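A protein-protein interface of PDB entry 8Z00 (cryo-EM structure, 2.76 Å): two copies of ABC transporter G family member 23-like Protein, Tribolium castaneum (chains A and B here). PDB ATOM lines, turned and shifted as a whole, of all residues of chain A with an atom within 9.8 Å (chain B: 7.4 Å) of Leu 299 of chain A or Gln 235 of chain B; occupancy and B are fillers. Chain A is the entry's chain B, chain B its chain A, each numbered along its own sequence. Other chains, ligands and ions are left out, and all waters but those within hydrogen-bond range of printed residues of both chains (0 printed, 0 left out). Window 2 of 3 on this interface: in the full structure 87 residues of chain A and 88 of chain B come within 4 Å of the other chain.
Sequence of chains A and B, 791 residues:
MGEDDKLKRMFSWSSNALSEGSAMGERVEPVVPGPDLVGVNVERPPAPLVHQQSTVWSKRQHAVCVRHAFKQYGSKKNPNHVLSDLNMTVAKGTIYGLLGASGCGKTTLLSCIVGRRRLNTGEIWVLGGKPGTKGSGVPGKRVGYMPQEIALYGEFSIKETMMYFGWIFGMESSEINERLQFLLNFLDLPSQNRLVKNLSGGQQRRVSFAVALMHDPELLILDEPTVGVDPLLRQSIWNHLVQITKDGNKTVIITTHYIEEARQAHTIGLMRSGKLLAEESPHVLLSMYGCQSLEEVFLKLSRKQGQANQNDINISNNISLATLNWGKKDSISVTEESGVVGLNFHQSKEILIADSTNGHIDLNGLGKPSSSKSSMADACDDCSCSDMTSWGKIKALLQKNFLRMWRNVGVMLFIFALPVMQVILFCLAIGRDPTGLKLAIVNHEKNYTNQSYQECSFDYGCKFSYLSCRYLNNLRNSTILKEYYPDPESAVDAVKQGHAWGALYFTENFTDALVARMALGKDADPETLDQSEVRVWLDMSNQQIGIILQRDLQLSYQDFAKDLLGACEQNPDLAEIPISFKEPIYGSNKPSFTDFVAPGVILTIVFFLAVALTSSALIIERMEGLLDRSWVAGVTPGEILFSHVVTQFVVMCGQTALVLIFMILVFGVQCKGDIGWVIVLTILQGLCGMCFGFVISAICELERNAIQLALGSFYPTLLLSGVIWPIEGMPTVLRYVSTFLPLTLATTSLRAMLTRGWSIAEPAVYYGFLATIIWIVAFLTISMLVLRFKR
Of the 17 printed residues of chain B, 5 touch a printed residue of chain A.
Printed residues of chain A that touch a printed residue of chain B: Ala 101, Arg 272, Glu 295 and Leu 299.
Hydrophobic or aromatic side chains of chain A within 4 Å of the printed part of chain B: Ala 101 and Leu 299.
Along chain A the printed residues that touch a printed residue of chain B span positions 101 to 299.
The side-chain carboxylate of Glu 295 of chain A lies within salt-bridge range of the guanidinium group of Arg 234 of chain B.
NE of Arg 234 of chain B is in salt-bridge range of OE2 of Glu 261 of chain B (2.5 Å).
N of Glu 295 of chain A sits close to OG of Ser 293 of chain A.
The backbone carbonyl oxygen (O) of Val 229 of chain B lies within hydrogen-bond range of the guanidinium group (NH1) of Arg 234 of chain B, 2.9 Å away.
Ala 101 of chain A touches Asp 230 of chain B.
CD1 of Leu 232 of chain B touches NH2 of Arg 272 of chain A, at 3.5 Å.
CB of Pro 231 of chain B touches CD2 of Leu 299 of chain A, 3.6 Å away.
Leu 299 of chain A touches Leu 232 of chain B.
Gln 235 of chain B touches Leu 299 of chain A (NE2 to CD1, 3.99 Å).
No position is printed for both chains.
Of chain A, only Leu 299 comes within 4 Å of Pro 231 of chain B.
No residue of chain A comes within 4 Å of Ser 236 of chain B.
Printed residues of chain A within 4 Å of Leu 232 of chain B: Arg 272 (3.5 Å) and Leu 299 (3.9 Å).
Printed residues of chain B within 4 Å of Ala 101 of chain A: Asp 230.
Printed residues of chain B within 4 Å of Glu 295 of chain A: Arg 234.
Printed residues of chain A within 4 Å of Asp 230 of chain B: Ala 101.
The nearest printed residue of chain B that does not touch Leu 299 of chain A is Asp 230 of chain B (6.7 Å).
The nearest printed residue of chain A that does not touch Arg 234 of chain B is Ile 259 of chain A (5.2 Å).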
ATOM      1  N   ALA A 101      10.586   3.779  36.400  1.00  0.00           N
ATOM      2  CA  ALA A 101      10.060   2.623  35.683  1.00  0.00           C
ATOM      3  C   ALA A 101       9.331   1.670  36.622  1.00  0.00           C
ATOM      4  O   ALA A 101       8.271   1.138  36.275  1.00  0.00           O
ATOM      5  CB  ALA A 101      11.191   1.899  34.954  1.00  0.00           C
ATOM      6  N   ILE A 259       2.731  10.373  33.524  1.00  0.00           N
ATOM      7  CA  ILE A 259       3.925  11.163  33.246  1.00  0.00           C
ATOM      8  C   ILE A 259       3.552  12.553  32.747  1.00  0.00           C
ATOM      9  O   ILE A 259       4.171  13.552  33.132  1.00  0.00           O
ATOM     10  CB  ILE A 259       4.829  10.422  32.246  1.00  0.00           C
ATOM     11  CG1 ILE A 259       4.970   8.953  32.652  1.00  0.00           C
ATOM     12  CG2 ILE A 259       6.191  11.096  32.160  1.00  0.00           C
ATOM     13  CD1 ILE A 259       6.142   8.245  32.013  1.00  0.00           C
ATOM     14  N   LEU A 270      13.991  11.693  36.724  1.00  0.00           N
ATOM     15  CA  LEU A 270      13.652  10.437  36.065  1.00  0.00           C
ATOM     16  C   LEU A 270      14.512   9.313  36.631  1.00  0.00           C
ATOM     17  O   LEU A 270      15.743   9.368  36.558  1.00  0.00           O
ATOM     18  CB  LEU A 270      13.842  10.555  34.554  1.00  0.00           C
ATOM     19  CG  LEU A 270      13.053  11.674  33.872  1.00  0.00           C
ATOM     20  CD1 LEU A 270      13.572  11.918  32.465  1.00  0.00           C
ATOM     21  CD2 LEU A 270      11.572  11.347  33.849  1.00  0.00           C
ATOM     22  N   MET A 271      13.859   8.291  37.174  1.00  0.00           N
ATOM     23  CA  MET A 271      14.522   7.196  37.866  1.00  0.00           C
ATOM     24  C   MET A 271      14.587   5.962  36.976  1.00  0.00           C
ATOM     25  O   MET A 271      13.596   5.587  36.345  1.00  0.00           O
ATOM     26  CB  MET A 271      13.781   6.862  39.161  1.00  0.00           C
ATOM     27  CG  MET A 271      14.279   5.623  39.872  1.00  0.00           C
ATOM     28  SD  MET A 271      14.172   5.779  41.661  1.00  0.00           S
ATOM     29  CE  MET A 271      15.892   6.036  42.062  1.00  0.00           C
ATOM     30  N   ARG A 272      15.760   5.331  36.934  1.00  0.00           N
ATOM     31  CA  ARG A 272      15.938   4.112  36.154  1.00  0.00           C
ATOM     32  C   ARG A 272      17.171   3.374  36.650  1.00  0.00           C
ATOM     33  O   ARG A 272      18.232   3.982  36.822  1.00  0.00           O
ATOM     34  CB  ARG A 272      16.071   4.424  34.661  1.00  0.00           C
ATOM     35  CG  ARG A 272      15.543   3.328  33.752  1.00  0.00           C
ATOM     36  CD  ARG A 272      16.444   3.130  32.547  1.00  0.00           C
ATOM     37  NE  ARG A 272      15.822   2.289  31.532  1.00  0.00           N
ATOM     38  CZ  ARG A 272      16.389   1.213  31.002  1.00  0.00           C
ATOM     39  NH1 ARG A 272      17.596   0.816  31.370  1.00  0.00           N
ATOM     40  NH2 ARG A 272      15.728   0.519  30.081  1.00  0.00           N
ATOM     41  N   LEU A 277      18.457   9.326  35.754  1.00  0.00           N
ATOM     42  CA  LEU A 277      18.957   9.673  34.429  1.00  0.00           C
ATOM     43  C   LEU A 277      19.045  11.183  34.251  1.00  0.00           C
ATOM     44  O   LEU A 277      20.003  11.690  33.659  1.00  0.00           O
ATOM     45  CB  LEU A 277      18.065   9.061  33.350  1.00  0.00           C
ATOM     46  CG  LEU A 277      17.738   7.573  33.473  1.00  0.00           C
ATOM     47  CD1 LEU A 277      16.901   7.122  32.290  1.00  0.00           C
ATOM     48  CD2 LEU A 277      19.012   6.756  33.573  1.00  0.00           C
ATOM     49  N   TYR A 289      15.474  18.490  23.899  1.00  0.00           N
ATOM     50  CA  TYR A 289      15.267  17.416  22.939  1.00  0.00           C
ATOM     51  C   TYR A 289      14.150  17.709  21.946  1.00  0.00           C
ATOM     52  O   TYR A 289      13.864  16.863  21.093  1.00  0.00           O
ATOM     53  CB  TYR A 289      14.979  16.105  23.676  1.00  0.00           C
ATOM     54  CG  TYR A 289      16.107  15.655  24.578  1.00  0.00           C
ATOM     55  CD1 TYR A 289      17.357  15.350  24.059  1.00  0.00           C
ATOM     56  CD2 TYR A 289      15.920  15.540  25.947  1.00  0.00           C
ATOM     57  CE1 TYR A 289      18.390  14.941  24.881  1.00  0.00           C
ATOM     58  CE2 TYR A 289      16.946  15.131  26.777  1.00  0.00           C
ATOM     59  CZ  TYR A 289      18.179  14.833  26.239  1.00  0.00           C
ATOM     60  OH  TYR A 289      19.206  14.425  27.058  1.00  0.00           O
ATOM     61  N   CYS A 291      10.866  17.818  22.219  1.00  0.00           N
ATOM     62  CA  CYS A 291       9.758  16.881  22.313  1.00  0.00           C
ATOM     63  C   CYS A 291       8.489  17.597  22.758  1.00  0.00           C
ATOM     64  O   CYS A 291       8.534  18.593  23.483  1.00  0.00           O
ATOM     65  CB  CYS A 291      10.079  15.745  23.287  1.00  0.00           C
ATOM     66  SG  CYS A 291      11.689  14.970  23.038  1.00  0.00           S
ATOM     67  N   SER A 293       6.130  15.851  24.419  1.00  0.00           N
ATOM     68  CA  SER A 293       5.619  15.088  25.547  1.00  0.00           C
ATOM     69  C   SER A 293       6.787  14.510  26.330  1.00  0.00           C
ATOM     70  O   SER A 293       7.841  14.203  25.768  1.00  0.00           O
ATOM     71  CB  SER A 293       4.679  13.968  25.089  1.00  0.00           C
ATOM     72  OG  SER A 293       5.381  12.746  24.947  1.00  0.00           O
ATOM     73  N   LEU A 294       6.584  14.363  27.640  1.00  0.00           N
ATOM     74  CA  LEU A 294       7.609  13.806  28.513  1.00  0.00           C
ATOM     75  C   LEU A 294       7.752  12.297  28.370  1.00  0.00           C
ATOM     76  O   LEU A 294       8.766  11.743  28.806  1.00  0.00           O
ATOM     77  CB  LEU A 294       7.301  14.147  29.972  1.00  0.00           C
ATOM     78  CG  LEU A 294       7.805  15.491  30.497  1.00  0.00           C
ATOM     79  CD1 LEU A 294       7.138  15.820  31.821  1.00  0.00           C
ATOM     80  CD2 LEU A 294       9.317  15.469  30.647  1.00  0.00           C
ATOM     81  N   GLU A 295       6.760  11.625  27.779  1.00  0.00           N
ATOM     82  CA  GLU A 295       6.821  10.173  27.649  1.00  0.00           C
ATOM     83  C   GLU A 295       7.990   9.737  26.777  1.00  0.00           C
ATOM     84  O   GLU A 295       8.710   8.791  27.119  1.00  0.00           O
ATOM     85  CB  GLU A 295       5.505   9.644  27.079  1.00  0.00           C
ATOM     86  CG  GLU A 295       5.379   8.128  27.090  1.00  0.00           C
ATOM     87  CD  GLU A 295       5.524   7.534  28.476  1.00  0.00           C
ATOM     88  OE1 GLU A 295       4.501   7.410  29.178  1.00  0.00           O
ATOM     89  OE2 GLU A 295       6.661   7.185  28.861  1.00  0.00           O
ATOM     90  N   GLU A 296       8.197  10.411  25.647  1.00  0.00           N
ATOM     91  CA  GLU A 296       9.264  10.043  24.727  1.00  0.00           C
ATOM     92  C   GLU A 296      10.636  10.522  25.176  1.00  0.00           C
ATOM     93  O   GLU A 296      11.641  10.093  24.600  1.00  0.00           O
ATOM     94  CB  GLU A 296       8.951  10.574  23.326  1.00  0.00           C
ATOM     95  CG  GLU A 296       8.095  11.827  23.303  1.00  0.00           C
ATOM     96  CD  GLU A 296       8.022  12.449  21.923  1.00  0.00           C
ATOM     97  OE1 GLU A 296       7.852  11.690  20.944  1.00  0.00           O
ATOM     98  OE2 GLU A 296       8.124  13.689  21.818  1.00  0.00           O
ATOM     99  N   VAL A 297      10.706  11.411  26.169  1.00  0.00           N
ATOM    100  CA  VAL A 297      11.995  11.750  26.760  1.00  0.00           C
ATOM    101  C   VAL A 297      12.532  10.576  27.569  1.00  0.00           C
ATOM    102  O   VAL A 297      13.731  10.278  27.535  1.00  0.00           O
ATOM    103  CB  VAL A 297      11.874  13.023  27.613  1.00  0.00           C
ATOM    104  CG1 VAL A 297      13.249  13.536  27.999  1.00  0.00           C
ATOM    105  CG2 VAL A 297      11.096  14.088  26.862  1.00  0.00           C
ATOM    106  N   PHE A 298      11.652   9.884  28.298  1.00  0.00           N
ATOM    107  CA  PHE A 298      12.059   8.720  29.079  1.00  0.00           C
ATOM    108  C   PHE A 298      12.604   7.606  28.195  1.00  0.00           C
ATOM    109  O   PHE A 298      13.379   6.770  28.672  1.00  0.00           O
ATOM    110  CB  PHE A 298      10.874   8.208  29.902  1.00  0.00           C
ATOM    111  CG  PHE A 298      11.250   7.672  31.258  1.00  0.00           C
ATOM    112  CD1 PHE A 298      12.300   6.784  31.408  1.00  0.00           C
ATOM    113  CD2 PHE A 298      10.544   8.058  32.384  1.00  0.00           C
ATOM    114  CE1 PHE A 298      12.642   6.295  32.652  1.00  0.00           C
ATOM    115  CE2 PHE A 298      10.882   7.571  33.631  1.00  0.00           C
ATOM    116  CZ  PHE A 298      11.933   6.689  33.764  1.00  0.00           C
ATOM    117  N   LEU A 299      12.234   7.584  26.915  1.00  0.00           N
ATOM    118  CA  LEU A 299      12.710   6.563  25.982  1.00  0.00           C
ATOM    119  C   LEU A 299      14.174   6.849  25.659  1.00  0.00           C
ATOM    120  O   LEU A 299      14.535   7.309  24.573  1.00  0.00           O
ATOM    121  CB  LEU A 299      11.853   6.542  24.723  1.00  0.00           C
ATOM    122  CG  LEU A 299      10.685   5.555  24.698  1.00  0.00           C
ATOM    123  CD1 LEU A 299      10.341   5.175  23.269  1.00  0.00           C
ATOM    124  CD2 LEU A 299      11.004   4.319  25.519  1.00  0.00           C
ATOM    125  N   LYS A 300      15.034   6.571  26.635  1.00  0.00           N
ATOM    126  CA  LYS A 300      16.476   6.764  26.513  1.00  0.00           C
ATOM    127  C   LYS A 300      17.114   5.393  26.322  1.00  0.00           C
ATOM    128  O   LYS A 300      17.265   4.628  27.278  1.00  0.00           O
ATOM    129  CB  LYS A 300      17.043   7.474  27.738  1.00  0.00           C
ATOM    130  CG  LYS A 300      16.747   8.961  27.788  1.00  0.00           C
ATOM    131  CD  LYS A 300      17.167   9.555  29.123  1.00  0.00           C
ATOM    132  CE  LYS A 300      16.352  10.790  29.461  1.00  0.00           C
ATOM    133  NZ  LYS A 300      17.024  12.035  29.004  1.00  0.00           N
ATOM    134  N   LEU A 301      17.485   5.085  25.077  1.00  0.00           N
ATOM    135  CA  LEU A 301      18.202   3.852  24.792  1.00  0.00           C
ATOM    136  C   LEU A 301      19.655   3.905  25.248  1.00  0.00           C
ATOM    137  O   LEU A 301      20.319   2.863  25.249  1.00  0.00           O
ATOM    138  CB  LEU A 301      18.137   3.543  23.295  1.00  0.00           C
ATOM    139  CG  LEU A 301      16.755   3.189  22.740  1.00  0.00           C
ATOM    140  CD1 LEU A 301      16.131   4.382  22.034  1.00  0.00           C
ATOM    141  CD2 LEU A 301      16.841   1.992  21.806  1.00  0.00           C
ATOM    142  N   SER A 302      20.150   5.082  25.627  1.00  0.00           N
ATOM    143  CA  SER A 302      21.516   5.259  26.115  1.00  0.00           C
ATOM    144  C   SER A 302      22.548   4.774  25.101  1.00  0.00           C
ATOM    145  O   SER A 302      23.069   5.559  24.307  1.00  0.00           O
ATOM    146  CB  SER A 302      21.709   4.536  27.450  1.00  0.00           C
ATOM    147  OG  SER A 302      22.941   4.893  28.051  1.00  0.00           O
ATOM    148  N   PHE B 186      11.643 -13.733  25.465  1.00  0.00           N
ATOM    149  CA  PHE B 186      10.864 -12.553  25.104  1.00  0.00           C
ATOM    150  C   PHE B 186      10.646 -11.625  26.293  1.00  0.00           C
ATOM    151  O   PHE B 186      10.722 -10.400  26.151  1.00  0.00           O
ATOM    152  CB  PHE B 186       9.528 -12.993  24.502  1.00  0.00           C
ATOM    153  CG  PHE B 186       8.516 -11.892  24.380  1.00  0.00           C
ATOM    154  CD1 PHE B 186       8.777 -10.769  23.615  1.00  0.00           C
ATOM    155  CD2 PHE B 186       7.290 -11.991  25.015  1.00  0.00           C
ATOM    156  CE1 PHE B 186       7.842  -9.762  23.498  1.00  0.00           C
ATOM    157  CE2 PHE B 186       6.351 -10.987  24.903  1.00  0.00           C
ATOM    158  CZ  PHE B 186       6.627  -9.871  24.142  1.00  0.00           C
ATOM    159  N   THR B 226       1.075  -4.384  31.806  1.00  0.00           N
ATOM    160  CA  THR B 226       2.250  -3.527  31.943  1.00  0.00           C
ATOM    161  C   THR B 226       1.908  -2.408  32.921  1.00  0.00           C
ATOM    162  O   THR B 226       1.170  -1.479  32.578  1.00  0.00           O
ATOM    163  CB  THR B 226       2.679  -2.968  30.590  1.00  0.00           C
ATOM    164  OG1 THR B 226       1.651  -2.113  30.077  1.00  0.00           O
ATOM    165  CG2 THR B 226       2.926  -4.094  29.599  1.00  0.00           C
ATOM    166  N   VAL B 229       6.454  -2.088  34.246  1.00  0.00           N
ATOM    167  CA  VAL B 229       7.359  -2.570  33.211  1.00  0.00           C
ATOM    168  C   VAL B 229       8.107  -1.394  32.596  1.00  0.00           C
ATOM    169  O   VAL B 229       7.577  -0.287  32.466  1.00  0.00           O
ATOM    170  CB  VAL B 229       6.575  -3.368  32.148  1.00  0.00           C
ATOM    171  CG1 VAL B 229       7.520  -4.041  31.171  1.00  0.00           C
ATOM    172  CG2 VAL B 229       5.687  -4.400  32.818  1.00  0.00           C
ATOM    173  N   ASP B 230       9.361  -1.638  32.230  1.00  0.00           N
ATOM    174  CA  ASP B 230      10.165  -0.609  31.589  1.00  0.00           C
ATOM    175  C   ASP B 230       9.565  -0.251  30.231  1.00  0.00           C
ATOM    176  O   ASP B 230       9.019  -1.123  29.545  1.00  0.00           O
ATOM    177  CB  ASP B 230      11.604  -1.094  31.417  1.00  0.00           C
ATOM    178  CG  ASP B 230      12.352  -1.179  32.729  1.00  0.00           C
ATOM    179  OD1 ASP B 230      11.870  -0.604  33.726  1.00  0.00           O
ATOM    180  OD2 ASP B 230      13.423  -1.821  32.764  1.00  0.00           O
ATOM    181  N   PRO B 231       9.636   1.018  29.816  1.00  0.00           N
ATOM    182  CA  PRO B 231       9.084   1.387  28.500  1.00  0.00           C
ATOM    183  C   PRO B 231       9.733   0.650  27.342  1.00  0.00           C
ATOM    184  O   PRO B 231       9.065   0.397  26.330  1.00  0.00           O
ATOM    185  CB  PRO B 231       9.337   2.901  28.427  1.00  0.00           C
ATOM    186  CG  PRO B 231      10.407   3.168  29.435  1.00  0.00           C
ATOM    187  CD  PRO B 231      10.179   2.182  30.533  1.00  0.00           C
ATOM    188  N   LEU B 232      11.016   0.300  27.459  1.00  0.00           N
ATOM    189  CA  LEU B 232      11.669  -0.477  26.411  1.00  0.00           C
ATOM    190  C   LEU B 232      11.003  -1.836  26.239  1.00  0.00           C
ATOM    191  O   LEU B 232      10.792  -2.295  25.110  1.00  0.00           O
ATOM    192  CB  LEU B 232      13.155  -0.644  26.731  1.00  0.00           C
ATOM    193  CG  LEU B 232      14.029   0.607  26.631  1.00  0.00           C
ATOM    194  CD1 LEU B 232      15.501   0.229  26.624  1.00  0.00           C
ATOM    195  CD2 LEU B 232      13.675   1.420  25.396  1.00  0.00           C
ATOM    196  N   LEU B 233      10.666  -2.496  27.349  1.00  0.00           N
ATOM    197  CA  LEU B 233       9.937  -3.757  27.266  1.00  0.00           C
ATOM    198  C   LEU B 233       8.476  -3.536  26.902  1.00  0.00           C
ATOM    199  O   LEU B 233       7.863  -4.396  26.262  1.00  0.00           O
ATOM    200  CB  LEU B 233      10.049  -4.514  28.589  1.00  0.00           C
ATOM    201  CG  LEU B 233       9.709  -6.006  28.566  1.00  0.00           C
ATOM    202  CD1 LEU B 233      10.579  -6.739  27.560  1.00  0.00           C
ATOM    203  CD2 LEU B 233       9.863  -6.612  29.950  1.00  0.00           C
ATOM    204  N   ARG B 234       7.903  -2.399  27.305  1.00  0.00           N
ATOM    205  CA  ARG B 234       6.514  -2.103  26.968  1.00  0.00           C
ATOM    206  C   ARG B 234       6.325  -1.978  25.462  1.00  0.00           C
ATOM    207  O   ARG B 234       5.330  -2.466  24.909  1.00  0.00           O
ATOM    208  CB  ARG B 234       6.072  -0.819  27.669  1.00  0.00           C
ATOM    209  CG  ARG B 234       5.170  -1.043  28.862  1.00  0.00           C
ATOM    210  CD  ARG B 234       5.494  -0.082  29.989  1.00  0.00           C
ATOM    211  NE  ARG B 234       5.333   1.310  29.591  1.00  0.00           N
ATOM    212  CZ  ARG B 234       5.728   2.345  30.320  1.00  0.00           C
ATOM    213  NH1 ARG B 234       6.316   2.180  31.493  1.00  0.00           N
ATOM    214  NH2 ARG B 234       5.529   3.577  29.859  1.00  0.00           N
ATOM    215  N   GLN B 235       7.267  -1.318  24.785  1.00  0.00           N
ATOM    216  CA  GLN B 235       7.185  -1.192  23.334  1.00  0.00           C
ATOM    217  C   GLN B 235       7.218  -2.558  22.662  1.00  0.00           C
ATOM    218  O   GLN B 235       6.435  -2.824  21.743  1.00  0.00           O
ATOM    219  CB  GLN B 235       8.323  -0.314  22.820  1.00  0.00           C
ATOM    220  CG  GLN B 235       7.889   1.066  22.357  1.00  0.00           C
ATOM    221  CD  GLN B 235       8.835   1.656  21.331  1.00  0.00           C
ATOM    222  OE1 GLN B 235       9.916   1.119  21.087  1.00  0.00           O
ATOM    223  NE2 GLN B 235       8.433   2.766  20.724  1.00  0.00           N
ATOM    224  N   SER B 236       8.112  -3.440  23.115  1.00  0.00           N
ATOM    225  CA  SER B 236       8.190  -4.780  22.542  1.00  0.00           C
ATOM    226  C   SER B 236       6.919  -5.576  22.813  1.00  0.00           C
ATOM    227  O   SER B 236       6.447  -6.312  21.940  1.00  0.00           O
ATOM    228  CB  SER B 236       9.411  -5.515  23.091  1.00  0.00           C
ATOM    229  OG  SER B 236       9.231  -5.845  24.457  1.00  0.00           O
ATOM    230  N   ILE B 237       6.355  -5.445  24.014  1.00  0.00           N
ATOM    231  CA  ILE B 237       5.131  -6.170  24.349  1.00  0.00           C
ATOM    232  C   ILE B 237       3.985  -5.723  23.452  1.00  0.00           C
ATOM    233  O   ILE B 237       3.231  -6.546  22.916  1.00  0.00           O
ATOM    234  CB  ILE B 237       4.790  -5.984  25.838  1.00  0.00           C
ATOM    235  CG1 ILE B 237       5.708  -6.843  26.708  1.00  0.00           C
ATOM    236  CG2 ILE B 237       3.330  -6.319  26.103  1.00  0.00           C
ATOM    237  CD1 ILE B 237       5.508  -6.640  28.191  1.00  0.00           C
ATOM    238  N   TRP B 238       3.838  -4.408  23.269  1.00  0.00           N
ATOM    239  CA  TRP B 238       2.763  -3.909  22.418  1.00  0.00           C
ATOM    240  C   TRP B 238       2.988  -4.288  20.959  1.00  0.00           C
ATOM    241  O   TRP B 238       2.030  -4.595  20.238  1.00  0.00           O
ATOM    242  CB  TRP B 238       2.622  -2.397  22.578  1.00  0.00           C
ATOM    243  CG  TRP B 238       1.592  -2.020  23.596  1.00  0.00           C
ATOM    244  CD1 TRP B 238       1.804  -1.760  24.917  1.00  0.00           C
ATOM    245  CD2 TRP B 238       0.183  -1.877  23.381  1.00  0.00           C
ATOM    246  NE1 TRP B 238       0.617  -1.458  25.538  1.00  0.00           N
ATOM    247  CE2 TRP B 238      -0.393  -1.523  24.616  1.00  0.00           C
ATOM    248  CE3 TRP B 238      -0.646  -2.010  22.264  1.00  0.00           C
ATOM    249  CZ2 TRP B 238      -1.759  -1.299  24.764  1.00  0.00           C
ATOM    250  CZ3 TRP B 238      -1.999  -1.789  22.414  1.00  0.00           C
ATOM    251  CH2 TRP B 238      -2.543  -1.437  23.653  1.00  0.00           C
ATOM    252  N   ASN B 239       4.245  -4.285  20.506  1.00  0.00           N
ATOM    253  CA  ASN B 239       4.543  -4.733  19.149  1.00  0.00           C
ATOM    254  C   ASN B 239       4.178  -6.200  18.962  1.00  0.00           C
ATOM    255  O   ASN B 239       3.628  -6.583  17.923  1.00  0.00           O
ATOM    256  CB  ASN B 239       6.021  -4.507  18.837  1.00  0.00           C
ATOM    257  CG  ASN B 239       6.288  -3.148  18.230  1.00  0.00           C
ATOM    258  OD1 ASN B 239       5.362  -2.424  17.870  1.00  0.00           O
ATOM    259  ND2 ASN B 239       7.562  -2.794  18.112  1.00  0.00           N
ATOM    260  N   HIS B 240       4.476  -7.036  19.958  1.00  0.00           N
ATOM    261  CA  HIS B 240       4.115  -8.448  19.879  1.00  0.00           C
ATOM    262  C   HIS B 240       2.604  -8.631  19.846  1.00  0.00           C
ATOM    263  O   HIS B 240       2.088  -9.463  19.089  1.00  0.00           O
ATOM    264  CB  HIS B 240       4.723  -9.208  21.058  1.00  0.00           C
ATOM    265  CG  HIS B 240       4.242 -10.620  21.181  1.00  0.00           C
ATOM    266  ND1 HIS B 240       4.770 -11.653  20.436  1.00  0.00           N
ATOM    267  CD2 HIS B 240       3.284 -11.170  21.962  1.00  0.00           C
ATOM    268  CE1 HIS B 240       4.157 -12.779  20.754  1.00  0.00           C
ATOM    269  NE2 HIS B 240       3.250 -12.514  21.677  1.00  0.00           N
ATOM    270  N   LEU B 241       1.877  -7.869  20.668  1.00  0.00           N
ATOM    271  CA  LEU B 241       0.420  -7.954  20.651  1.00  0.00           C
ATOM    272  C   LEU B 241      -0.139  -7.558  19.288  1.00  0.00           C
ATOM    273  O   LEU B 241      -1.025  -8.234  18.748  1.00  0.00           O
ATOM    274  CB  LEU B 241      -0.171  -7.069  21.747  1.00  0.00           C
ATOM    275  CG  LEU B 241      -0.130  -7.603  23.179  1.00  0.00           C
ATOM    276  CD1 LEU B 241      -0.706  -6.575  24.138  1.00  0.00           C
ATOM    277  CD2 LEU B 241      -0.880  -8.918  23.288  1.00  0.00           C
ATOM    278  N   GLU B 261      -0.368   4.841  25.367  1.00  0.00           N
ATOM    279  CA  GLU B 261       0.115   3.561  24.860  1.00  0.00           C
ATOM    280  C   GLU B 261      -0.952   2.816  24.069  1.00  0.00           C
ATOM    281  O   GLU B 261      -0.613   1.926  23.283  1.00  0.00           O
ATOM    282  CB  GLU B 261       0.609   2.690  26.015  1.00  0.00           C
ATOM    283  CG  GLU B 261       2.122   2.618  26.136  1.00  0.00           C
ATOM    284  CD  GLU B 261       2.572   1.775  27.311  1.00  0.00           C
ATOM    285  OE1 GLU B 261       1.765   0.957  27.802  1.00  0.00           O
ATOM    286  OE2 GLU B 261       3.734   1.929  27.744  1.00  0.00           O
ATOM    287  N   GLN B 264      -2.035   2.196  19.557  1.00  0.00           N
ATOM    288  CA  GLN B 264      -1.959   1.061  18.648  1.00  0.00           C
ATOM    289  C   GLN B 264      -3.195   0.174  18.701  1.00  0.00           C
ATOM    290  O   GLN B 264      -3.369  -0.669  17.815  1.00  0.00           O
ATOM    291  CB  GLN B 264      -0.716   0.225  18.956  1.00  0.00           C
ATOM    292  CG  GLN B 264       0.456   0.498  18.035  1.00  0.00           C
ATOM    293  CD  GLN B 264       1.772   0.034  18.620  1.00  0.00           C
ATOM    294  OE1 GLN B 264       2.179   0.482  19.691  1.00  0.00           O
ATOM    295  NE2 GLN B 264       2.445  -0.870  17.919  1.00  0.00           N
